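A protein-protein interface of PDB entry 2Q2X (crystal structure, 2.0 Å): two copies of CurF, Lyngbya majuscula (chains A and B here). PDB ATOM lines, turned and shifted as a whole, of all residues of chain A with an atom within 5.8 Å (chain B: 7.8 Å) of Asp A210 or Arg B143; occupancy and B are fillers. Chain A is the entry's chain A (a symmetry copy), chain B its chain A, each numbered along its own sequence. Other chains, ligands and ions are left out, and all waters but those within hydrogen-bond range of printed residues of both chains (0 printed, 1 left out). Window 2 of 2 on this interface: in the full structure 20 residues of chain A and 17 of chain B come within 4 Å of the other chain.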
ATOM      1  N   GLU A 144      20.067  -4.675  -3.185  1.00  0.00           N
ATOM      2  CA  GLU A 144      21.159  -5.197  -2.372  1.00  0.00           C
ATOM      3  C   GLU A 144      20.781  -5.334  -0.901  1.00  0.00           C
ATOM      4  O   GLU A 144      21.076  -6.357  -0.285  1.00  0.00           O
ATOM      5  CB  GLU A 144      22.410  -4.338  -2.536  1.00  0.00           C
ATOM      6  CG  GLU A 144      23.583  -4.679  -1.591  1.00  0.00           C
ATOM      7  CD  GLU A 144      24.371  -5.930  -2.002  1.00  0.00           C
ATOM      8  OE1 GLU A 144      23.992  -6.607  -2.998  1.00  0.00           O
ATOM      9  OE2 GLU A 144      25.387  -6.227  -1.326  1.00  0.00           O
ATOM     10  N   HIS A 206      36.585  -3.096   1.772  1.00  0.00           N
ATOM     11  CA  HIS A 206      36.547  -4.403   1.134  1.00  0.00           C
ATOM     12  C   HIS A 206      35.109  -4.816   0.888  1.00  0.00           C
ATOM     13  O   HIS A 206      34.777  -5.271  -0.208  1.00  0.00           O
ATOM     14  CB  HIS A 206      37.265  -5.445   2.018  1.00  0.00           C
ATOM     15  CG  HIS A 206      37.152  -6.847   1.518  1.00  0.00           C
ATOM     16  ND1 HIS A 206      37.663  -7.248   0.301  1.00  0.00           N
ATOM     17  CD2 HIS A 206      36.584  -7.946   2.069  1.00  0.00           C
ATOM     18  CE1 HIS A 206      37.413  -8.532   0.123  1.00  0.00           C
ATOM     19  NE2 HIS A 206      36.756  -8.978   1.179  1.00  0.00           N
ATOM     20  N   LEU A 207      34.264  -4.645   1.903  1.00  0.00           N
ATOM     21  CA  LEU A 207      32.880  -5.105   1.842  1.00  0.00           C
ATOM     22  C   LEU A 207      32.051  -4.244   0.906  1.00  0.00           C
ATOM     23  O   LEU A 207      31.101  -4.728   0.305  1.00  0.00           O
ATOM     24  CB  LEU A 207      32.247  -5.148   3.232  1.00  0.00           C
ATOM     25  CG  LEU A 207      32.805  -6.145   4.256  1.00  0.00           C
ATOM     26  CD1 LEU A 207      32.053  -6.026   5.575  1.00  0.00           C
ATOM     27  CD2 LEU A 207      32.791  -7.582   3.770  1.00  0.00           C
ATOM     28  N   SER A 208      32.448  -2.985   0.764  1.00  0.00           N
ATOM     29  CA  SER A 208      31.772  -1.996  -0.093  1.00  0.00           C
ATOM     30  C   SER A 208      32.171  -2.008  -1.576  1.00  0.00           C
ATOM     31  O   SER A 208      31.540  -1.327  -2.394  1.00  0.00           O
ATOM     32  CB  SER A 208      32.031  -0.589   0.461  1.00  0.00           C
ATOM     33  OG  SER A 208      31.448  -0.464   1.748  1.00  0.00           O
ATOM     34  N   ALA A 209      33.217  -2.761  -1.912  1.00  0.00           N
ATOM     35  CA  ALA A 209      33.862  -2.668  -3.224  1.00  0.00           C
ATOM     36  C   ALA A 209      32.935  -3.038  -4.381  1.00  0.00           C
ATOM     37  O   ALA A 209      32.920  -2.362  -5.418  1.00  0.00           O
ATOM     38  CB  ALA A 209      35.121  -3.520  -3.256  1.00  0.00           C
ATOM     39  N   ASP A 210      32.166  -4.107  -4.207  1.00  0.00           N
ATOM     40  CA  ASP A 210      31.213  -4.529  -5.235  1.00  0.00           C
ATOM     41  C   ASP A 210      30.212  -3.418  -5.557  1.00  0.00           C
ATOM     42  O   ASP A 210      30.137  -2.972  -6.712  1.00  0.00           O
ATOM     43  CB  ASP A 210      30.520  -5.831  -4.834  1.00  0.00           C
ATOM     44  CG  ASP A 210      31.394  -7.065  -5.080  1.00  0.00           C
ATOM     45  OD1 ASP A 210      32.419  -6.965  -5.811  1.00  0.00           O
ATOM     46  OD2 ASP A 210      31.052  -8.148  -4.543  1.00  0.00           O
ATOM     47  N   ILE A 211      29.498  -2.931  -4.538  1.00  0.00           N
ATOM     48  CA  ILE A 211      28.553  -1.818  -4.718  1.00  0.00           C
ATOM     49  C   ILE A 211      29.254  -0.554  -5.238  1.00  0.00           C
ATOM     50  O   ILE A 211      28.746   0.104  -6.144  1.00  0.00           O
ATOM     51  CB  ILE A 211      27.771  -1.496  -3.420  1.00  0.00           C
ATOM     52  CG1 ILE A 211      26.846  -2.663  -3.015  1.00  0.00           C
ATOM     53  CG2 ILE A 211      26.985  -0.165  -3.551  1.00  0.00           C
ATOM     54  CD1 ILE A 211      25.701  -2.990  -4.008  1.00  0.00           C
ATOM     55  N   LYS A 212      30.422  -0.234  -4.673  1.00  0.00           N
ATOM     56  CA  LYS A 212      31.190   0.956  -5.054  1.00  0.00           C
ATOM     57  C   LYS A 212      31.547   0.928  -6.538  1.00  0.00           C
ATOM     58  O   LYS A 212      31.502   1.948  -7.213  1.00  0.00           O
ATOM     59  CB  LYS A 212      32.470   1.043  -4.213  1.00  0.00           C
ATOM     60  CG  LYS A 212      32.951   2.456  -3.892  1.00  0.00           C
ATOM     61  CD  LYS A 212      32.402   2.921  -2.530  1.00  0.00           C
ATOM     62  CE  LYS A 212      32.739   4.388  -2.249  1.00  0.00           C
ATOM     63  NZ  LYS A 212      34.119   4.601  -1.707  1.00  0.00           N
ATOM     64  N   ALA A 213      31.882  -0.256  -7.040  1.00  0.00           N
ATOM     65  CA  ALA A 213      32.239  -0.443  -8.440  1.00  0.00           C
ATOM     66  C   ALA A 213      31.059  -0.226  -9.397  1.00  0.00           C
ATOM     67  O   ALA A 213      31.254   0.232 -10.533  1.00  0.00           O
ATOM     68  CB  ALA A 213      32.834  -1.829  -8.647  1.00  0.00           C
ATOM     69  N   LYS A 214      29.855  -0.592  -8.951  1.00  0.00           N
ATOM     70  CA  LYS A 214      28.633  -0.448  -9.760  1.00  0.00           C
ATOM     71  C   LYS A 214      27.970   0.927  -9.639  1.00  0.00           C
ATOM     72  O   LYS A 214      27.158   1.296 -10.475  1.00  0.00           O
ATOM     73  CB  LYS A 214      27.609  -1.520  -9.386  1.00  0.00           C
ATOM     74  CG  LYS A 214      28.156  -2.942  -9.460  1.00  0.00           C
ATOM     75  CD  LYS A 214      27.039  -3.939  -9.616  1.00  0.00           C
ATOM     76  CE  LYS A 214      27.451  -5.314  -9.128  1.00  0.00           C
ATOM     77  NZ  LYS A 214      26.594  -6.363  -9.757  1.00  0.00           N
ATOM     78  N   PHE A 215      28.316   1.667  -8.594  1.00  0.00           N
ATOM     79  CA  PHE A 215      27.579   2.872  -8.221  1.00  0.00           C
ATOM     80  C   PHE A 215      27.583   4.036  -9.243  1.00  0.00           C
ATOM     81  O   PHE A 215      26.509   4.557  -9.574  1.00  0.00           O
ATOM     82  CB  PHE A 215      28.031   3.371  -6.842  1.00  0.00           C
ATOM     83  CG  PHE A 215      27.045   4.292  -6.187  1.00  0.00           C
ATOM     84  CD1 PHE A 215      25.989   3.777  -5.437  1.00  0.00           C
ATOM     85  CD2 PHE A 215      27.153   5.665  -6.326  1.00  0.00           C
ATOM     86  CE1 PHE A 215      25.069   4.631  -4.832  1.00  0.00           C
ATOM     87  CE2 PHE A 215      26.232   6.521  -5.717  1.00  0.00           C
ATOM     88  CZ  PHE A 215      25.195   5.999  -4.981  1.00  0.00           C
ATOM     89  N   LEU B 110      30.668 -23.757   4.889  1.00  0.00           N
ATOM     90  CA  LEU B 110      29.928 -22.890   3.972  1.00  0.00           C
ATOM     91  C   LEU B 110      30.352 -22.980   2.490  1.00  0.00           C
ATOM     92  O   LEU B 110      29.602 -22.561   1.602  1.00  0.00           O
ATOM     93  CB  LEU B 110      29.942 -21.448   4.453  1.00  0.00           C
ATOM     94  CG  LEU B 110      29.207 -21.191   5.780  1.00  0.00           C
ATOM     95  CD1 LEU B 110      29.226 -19.717   6.049  1.00  0.00           C
ATOM     96  CD2 LEU B 110      27.771 -21.685   5.746  1.00  0.00           C
ATOM     97  N   ALA B 137      38.100 -16.014   1.278  1.00  0.00           N
ATOM     98  CA  ALA B 137      36.942 -15.450   0.571  1.00  0.00           C
ATOM     99  C   ALA B 137      35.677 -15.491   1.427  1.00  0.00           C
ATOM    100  O   ALA B 137      34.580 -15.808   0.946  1.00  0.00           O
ATOM    101  CB  ALA B 137      36.725 -16.100  -0.795  1.00  0.00           C
ATOM    102  N   THR B 138      35.849 -15.137   2.697  1.00  0.00           N
ATOM    103  CA  THR B 138      34.766 -15.079   3.665  1.00  0.00           C
ATOM    104  C   THR B 138      33.620 -14.169   3.198  1.00  0.00           C
ATOM    105  O   THR B 138      32.463 -14.591   3.167  1.00  0.00           O
ATOM    106  CB  THR B 138      35.307 -14.603   5.029  1.00  0.00           C
ATOM    107  OG1 THR B 138      36.148 -15.623   5.580  1.00  0.00           O
ATOM    108  CG2 THR B 138      34.156 -14.295   6.011  1.00  0.00           C
ATOM    109  N   SER B 139      33.957 -12.933   2.835  1.00  0.00           N
ATOM    110  CA  SER B 139      32.978 -11.953   2.340  1.00  0.00           C
ATOM    111  C   SER B 139      32.131 -12.541   1.196  1.00  0.00           C
ATOM    112  O   SER B 139      30.900 -12.493   1.231  1.00  0.00           O
ATOM    113  CB  SER B 139      33.717 -10.707   1.858  1.00  0.00           C
ATOM    114  OG  SER B 139      32.825  -9.740   1.348  1.00  0.00           O
ATOM    115  N   LEU B 140      32.804 -13.103   0.193  1.00  0.00           N
ATOM    116  CA  LEU B 140      32.126 -13.694  -0.974  1.00  0.00           C
ATOM    117  C   LEU B 140      31.156 -14.787  -0.576  1.00  0.00           C
ATOM    118  O   LEU B 140      29.981 -14.712  -0.909  1.00  0.00           O
ATOM    119  CB  LEU B 140      33.146 -14.254  -1.980  1.00  0.00           C
ATOM    120  CG  LEU B 140      32.620 -14.849  -3.290  1.00  0.00           C
ATOM    121  CD1 LEU B 140      32.064 -13.753  -4.223  1.00  0.00           C
ATOM    122  CD2 LEU B 140      33.736 -15.647  -3.980  1.00  0.00           C
ATOM    123  N   ILE B 141      31.648 -15.799   0.136  1.00  0.00           N
ATOM    124  CA  ILE B 141      30.863 -16.973   0.469  1.00  0.00           C
ATOM    125  C   ILE B 141      29.754 -16.632   1.476  1.00  0.00           C
ATOM    126  O   ILE B 141      28.606 -17.081   1.319  1.00  0.00           O
ATOM    127  CB  ILE B 141      31.792 -18.129   0.980  1.00  0.00           C
ATOM    128  CG1 ILE B 141      32.845 -18.507  -0.093  1.00  0.00           C
ATOM    129  CG2 ILE B 141      31.012 -19.360   1.419  1.00  0.00           C
ATOM    130  CD1 ILE B 141      32.298 -19.322  -1.335  1.00  0.00           C
ATOM    131  N   LEU B 142      30.070 -15.822   2.489  1.00  0.00           N
ATOM    132  CA  LEU B 142      29.060 -15.507   3.521  1.00  0.00           C
ATOM    133  C   LEU B 142      27.903 -14.667   2.988  1.00  0.00           C
ATOM    134  O   LEU B 142      26.731 -14.915   3.312  1.00  0.00           O
ATOM    135  CB  LEU B 142      29.666 -14.800   4.737  1.00  0.00           C
ATOM    136  CG  LEU B 142      30.051 -15.600   5.971  1.00  0.00           C
ATOM    137  CD1 LEU B 142      30.156 -14.625   7.137  1.00  0.00           C
ATOM    138  CD2 LEU B 142      29.042 -16.633   6.297  1.00  0.00           C
ATOM    139  N   ARG B 143      28.235 -13.683   2.169  1.00  0.00           N
ATOM    140  CA  ARG B 143      27.215 -12.864   1.551  1.00  0.00           C
ATOM    141  C   ARG B 143      26.353 -13.685   0.594  1.00  0.00           C
ATOM    142  O   ARG B 143      25.131 -13.542   0.591  1.00  0.00           O
ATOM    143  CB  ARG B 143      27.845 -11.645   0.896  1.00  0.00           C
ATOM    144  CG  ARG B 143      28.582 -10.808   1.939  1.00  0.00           C
ATOM    145  CD  ARG B 143      28.597  -9.327   1.625  1.00  0.00           C
ATOM    146  NE  ARG B 143      29.590  -8.981   0.610  1.00  0.00           N
ATOM    147  CZ  ARG B 143      29.861  -7.738   0.226  1.00  0.00           C
ATOM    148  NH1 ARG B 143      29.214  -6.711   0.770  1.00  0.00           N
ATOM    149  NH2 ARG B 143      30.780  -7.523  -0.706  1.00  0.00           N
ATOM    150  N   GLU B 144      26.981 -14.585  -0.158  1.00  0.00           N
ATOM    151  CA  GLU B 144      26.249 -15.474  -1.054  1.00  0.00           C
ATOM    152  C   GLU B 144      25.335 -16.438  -0.306  1.00  0.00           C
ATOM    153  O   GLU B 144      24.184 -16.622  -0.700  1.00  0.00           O
ATOM    154  CB  GLU B 144      27.213 -16.232  -1.964  1.00  0.00           C
ATOM    155  CG  GLU B 144      26.578 -17.337  -2.836  1.00  0.00           C
ATOM    156  CD  GLU B 144      25.818 -16.804  -4.060  1.00  0.00           C
ATOM    157  OE1 GLU B 144      25.707 -15.560  -4.232  1.00  0.00           O
ATOM    158  OE2 GLU B 144      25.339 -17.648  -4.860  1.00  0.00           O
ATOM    159  N   LYS B 145      25.820 -17.057   0.769  1.00  0.00           N
ATOM    160  CA  LYS B 145      25.033 -18.106   1.426  1.00  0.00           C
ATOM    161  C   LYS B 145      24.089 -17.585   2.518  1.00  0.00           C
ATOM    162  O   LYS B 145      23.018 -18.152   2.737  1.00  0.00           O
ATOM    163  CB  LYS B 145      25.920 -19.223   1.992  1.00  0.00           C
ATOM    164  CG  LYS B 145      27.050 -19.682   1.066  1.00  0.00           C
ATOM    165  CD  LYS B 145      26.633 -20.759   0.120  1.00  0.00           C
ATOM    166  CE  LYS B 145      27.787 -21.107  -0.802  1.00  0.00           C
ATOM    167  NZ  LYS B 145      27.955 -22.573  -0.875  1.00  0.00           N
ATOM    168  N   LEU B 146      24.483 -16.518   3.202  1.00  0.00           N
ATOM    169  CA  LEU B 146      23.717 -16.044   4.370  1.00  0.00           C
ATOM    170  C   LEU B 146      22.994 -14.730   4.130  1.00  0.00           C
ATOM    171  O   LEU B 146      22.126 -14.339   4.917  1.00  0.00           O
ATOM    172  CB  LEU B 146      24.620 -15.946   5.612  1.00  0.00           C
ATOM    173  CG  LEU B 146      25.314 -17.213   6.132  1.00  0.00           C
ATOM    174  CD1 LEU B 146      25.857 -16.949   7.519  1.00  0.00           C
ATOM    175  CD2 LEU B 146      24.415 -18.430   6.184  1.00  0.00           C
ATOM    176  N   GLY B 147      23.335 -14.065   3.035  1.00  0.00           N
ATOM    177  CA  GLY B 147      22.794 -12.737   2.726  1.00  0.00           C
ATOM    178  C   GLY B 147      23.748 -11.692   3.261  1.00  0.00           C
ATOM    179  O   GLY B 147      24.462 -11.954   4.225  1.00  0.00           O
ATOM    180  N   SER B 148      23.775 -10.515   2.645  1.00  0.00           N
ATOM    181  CA  SER B 148      24.767  -9.498   3.017  1.00  0.00           C
ATOM    182  C   SER B 148      24.686  -8.949   4.456  1.00  0.00           C
ATOM    183  O   SER B 148      25.725  -8.665   5.057  1.00  0.00           O
ATOM    184  CB  SER B 148      24.836  -8.365   1.981  1.00  0.00           C
ATOM    185  OG  SER B 148      23.551  -7.998   1.522  1.00  0.00           O
ATOM    186  N   GLU B 149      23.481  -8.819   5.008  1.00  0.00           N
ATOM    187  CA  GLU B 149      23.320  -8.182   6.313  1.00  0.00           C
ATOM    188  C   GLU B 149      23.734  -9.070   7.477  1.00  0.00           C
ATOM    189  O   GLU B 149      24.391  -8.600   8.396  1.00  0.00           O
ATOM    190  CB  GLU B 149      21.900  -7.637   6.516  1.00  0.00           C
ATOM    191  CG  GLU B 149      21.524  -6.489   5.535  1.00  0.00           C
ATOM    192  CD  GLU B 149      22.657  -5.480   5.286  1.00  0.00           C
ATOM    193  OE1 GLU B 149      23.122  -4.831   6.257  1.00  0.00           O
ATOM    194  OE2 GLU B 149      23.061  -5.329   4.109  1.00  0.00           O
ATOM    195  N   LEU B 150      23.359 -10.343   7.445  1.00  0.00           N
ATOM    196  CA  LEU B 150      23.850 -11.262   8.456  1.00  0.00           C
ATOM    197  C   LEU B 150      25.359 -11.433   8.301  1.00  0.00           C
ATOM    198  O   LEU B 150      26.072 -11.435   9.291  1.00  0.00           O
ATOM    199  CB  LEU B 150      23.171 -12.619   8.365  1.00  0.00           C
ATOM    200  CG  LEU B 150      22.704 -13.330   9.638  1.00  0.00           C
ATOM    201  CD1 LEU B 150      22.581 -14.809   9.314  1.00  0.00           C
ATOM    202  CD2 LEU B 150      23.607 -13.127  10.869  1.00  0.00           C
ATOM    203  N   ALA B 151      25.822 -11.577   7.056  1.00  0.00           N
ATOM    204  CA  ALA B 151      27.250 -11.745   6.768  1.00  0.00           C
ATOM    205  C   ALA B 151      28.057 -10.577   7.322  1.00  0.00           C
ATOM    206  O   ALA B 151      29.043 -10.785   8.010  1.00  0.00           O
ATOM    207  CB  ALA B 151      27.489 -11.887   5.279  1.00  0.00           C
ATOM    208  N   GLN B 152      27.614  -9.362   7.018  1.00  0.00           N
ATOM    209  CA  GLN B 152      28.261  -8.136   7.450  1.00  0.00           C
ATOM    210  C   GLN B 152      28.388  -8.051   8.980  1.00  0.00           C
ATOM    211  O   GLN B 152      29.473  -7.778   9.508  1.00  0.00           O
ATOM    212  CB  GLN B 152      27.515  -6.937   6.886  1.00  0.00           C
ATOM    213  CG  GLN B 152      28.120  -5.564   7.197  1.00  0.00           C
ATOM    214  CD  GLN B 152      28.201  -4.665   5.961  1.00  0.00           C
ATOM    215  OE1 GLN B 152      28.382  -5.147   4.839  1.00  0.00           O
ATOM    216  NE2 GLN B 152      28.070  -3.366   6.162  1.00  0.00           N
ATOM    217  N   ILE B 155      30.769 -10.715  10.216  1.00  0.00           N
ATOM    218  CA  ILE B 155      32.170 -10.422   9.844  1.00  0.00           C
ATOM    219  C   ILE B 155      32.763  -9.268  10.680  1.00  0.00           C
ATOM    220  O   ILE B 155      33.858  -9.397  11.218  1.00  0.00           O
ATOM    221  CB  ILE B 155      32.371 -10.172   8.322  1.00  0.00           C
ATOM    222  CG1 ILE B 155      32.034 -11.432   7.520  1.00  0.00           C
ATOM    223  CG2 ILE B 155      33.857  -9.797   8.041  1.00  0.00           C
ATOM    224  CD1 ILE B 155      31.806 -11.193   6.010  1.00  0.00           C
ATOM    225  N   ILE B 211      30.277 -18.190  -8.522  1.00  0.00           N
ATOM    226  CA  ILE B 211      31.204 -18.123  -7.381  1.00  0.00           C
ATOM    227  C   ILE B 211      32.629 -18.535  -7.780  1.00  0.00           C
ATOM    228  O   ILE B 211      33.592 -17.875  -7.396  1.00  0.00           O
ATOM    229  CB  ILE B 211      30.721 -18.974  -6.181  1.00  0.00           C
ATOM    230  CG1 ILE B 211      29.411 -18.416  -5.585  1.00  0.00           C
ATOM    231  CG2 ILE B 211      31.827 -19.105  -5.100  1.00  0.00           C
ATOM    232  CD1 ILE B 211      29.504 -17.001  -4.960  1.00  0.00           C
ATOM    233  N   LYS B 214      34.569 -15.790  -9.468  1.00  0.00           N
ATOM    234  CA  LYS B 214      34.960 -14.691  -8.571  1.00  0.00           C
ATOM    235  C   LYS B 214      35.990 -15.094  -7.511  1.00  0.00           C
ATOM    236  O   LYS B 214      36.636 -14.240  -6.922  1.00  0.00           O
ATOM    237  CB  LYS B 214      33.736 -14.107  -7.867  1.00  0.00           C
ATOM    238  CG  LYS B 214      32.629 -13.673  -8.823  1.00  0.00           C
ATOM    239  CD  LYS B 214      31.728 -12.656  -8.173  1.00  0.00           C
ATOM    240  CE  LYS B 214      30.357 -12.637  -8.821  1.00  0.00           C
ATOM    241  NZ  LYS B 214      29.685 -11.328  -8.567  1.00  0.00           N
ATOM    242  N   LYS B 221      42.406 -10.878  -2.833  1.00  0.00           N
ATOM    243  CA  LYS B 221      42.090  -9.570  -2.258  1.00  0.00           C
ATOM    244  C   LYS B 221      41.986  -9.598  -0.730  1.00  0.00           C
ATOM    245  O   LYS B 221      42.524  -8.727  -0.040  1.00  0.00           O
ATOM    246  CB  LYS B 221      40.800  -9.014  -2.859  1.00  0.00           C
ATOM    247  CG  LYS B 221      40.977  -8.336  -4.210  1.00  0.00           C
ATOM    248  CD  LYS B 221      39.611  -8.033  -4.819  1.00  0.00           C
ATOM    249  CE  LYS B 221      39.702  -7.509  -6.246  1.00  0.00           C
ATOM    250  NZ  LYS B 221      38.372  -7.630  -6.933  1.00  0.00           N
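The side-chain hydroxyl (OG) of Ser B148 is in hydrogen-bond range of the backbone carbonyl oxygen (O) of Glu A144 (3.5 Å).
The guanidinium group (NH2) of Arg B143 lies within salt-bridge range of the side-chain carboxylate (OD2) of Asp A210.
NH1 of Arg B143 sits at hydrogen-bond distance from O of Leu A207, 2.8 Å away.
Of the printed residues of chain B, Leu A207 touches Ser B139, Arg B143 and Gln B152.
No residue of chain B comes within 4 Å of Ala A209.
Asp A210 touches just one residue of chain B: Arg B143 (3.9 Å).
Phe A215 touches none of the printed residues of chain B.
Of the printed residues of chain A, Ser B139 touches His A206 and Leu A207.
Arg B143 touches two residues of chain A.
Of the printed residues of chain A, Ser B148 touches Glu A144.
Positions printed for both chains: 144, 211 and 214.
Among the printed residues, merely in contact across the chains: His A206 with Ser B139, Leu A207 with Ser B139 and Leu A207 with Gln B152.
The side-chain hydroxyl of Ser B139 sits at hydrogen-bond distance from the guanidinium group of Arg B143 (3.4 Å).
Of the 11 printed residues of chain A, 4 touch a printed residue of chain B.
Printed residues of chain A that touch a printed residue of chain B: Glu A144, His A206, Leu A207 and Asp A210.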
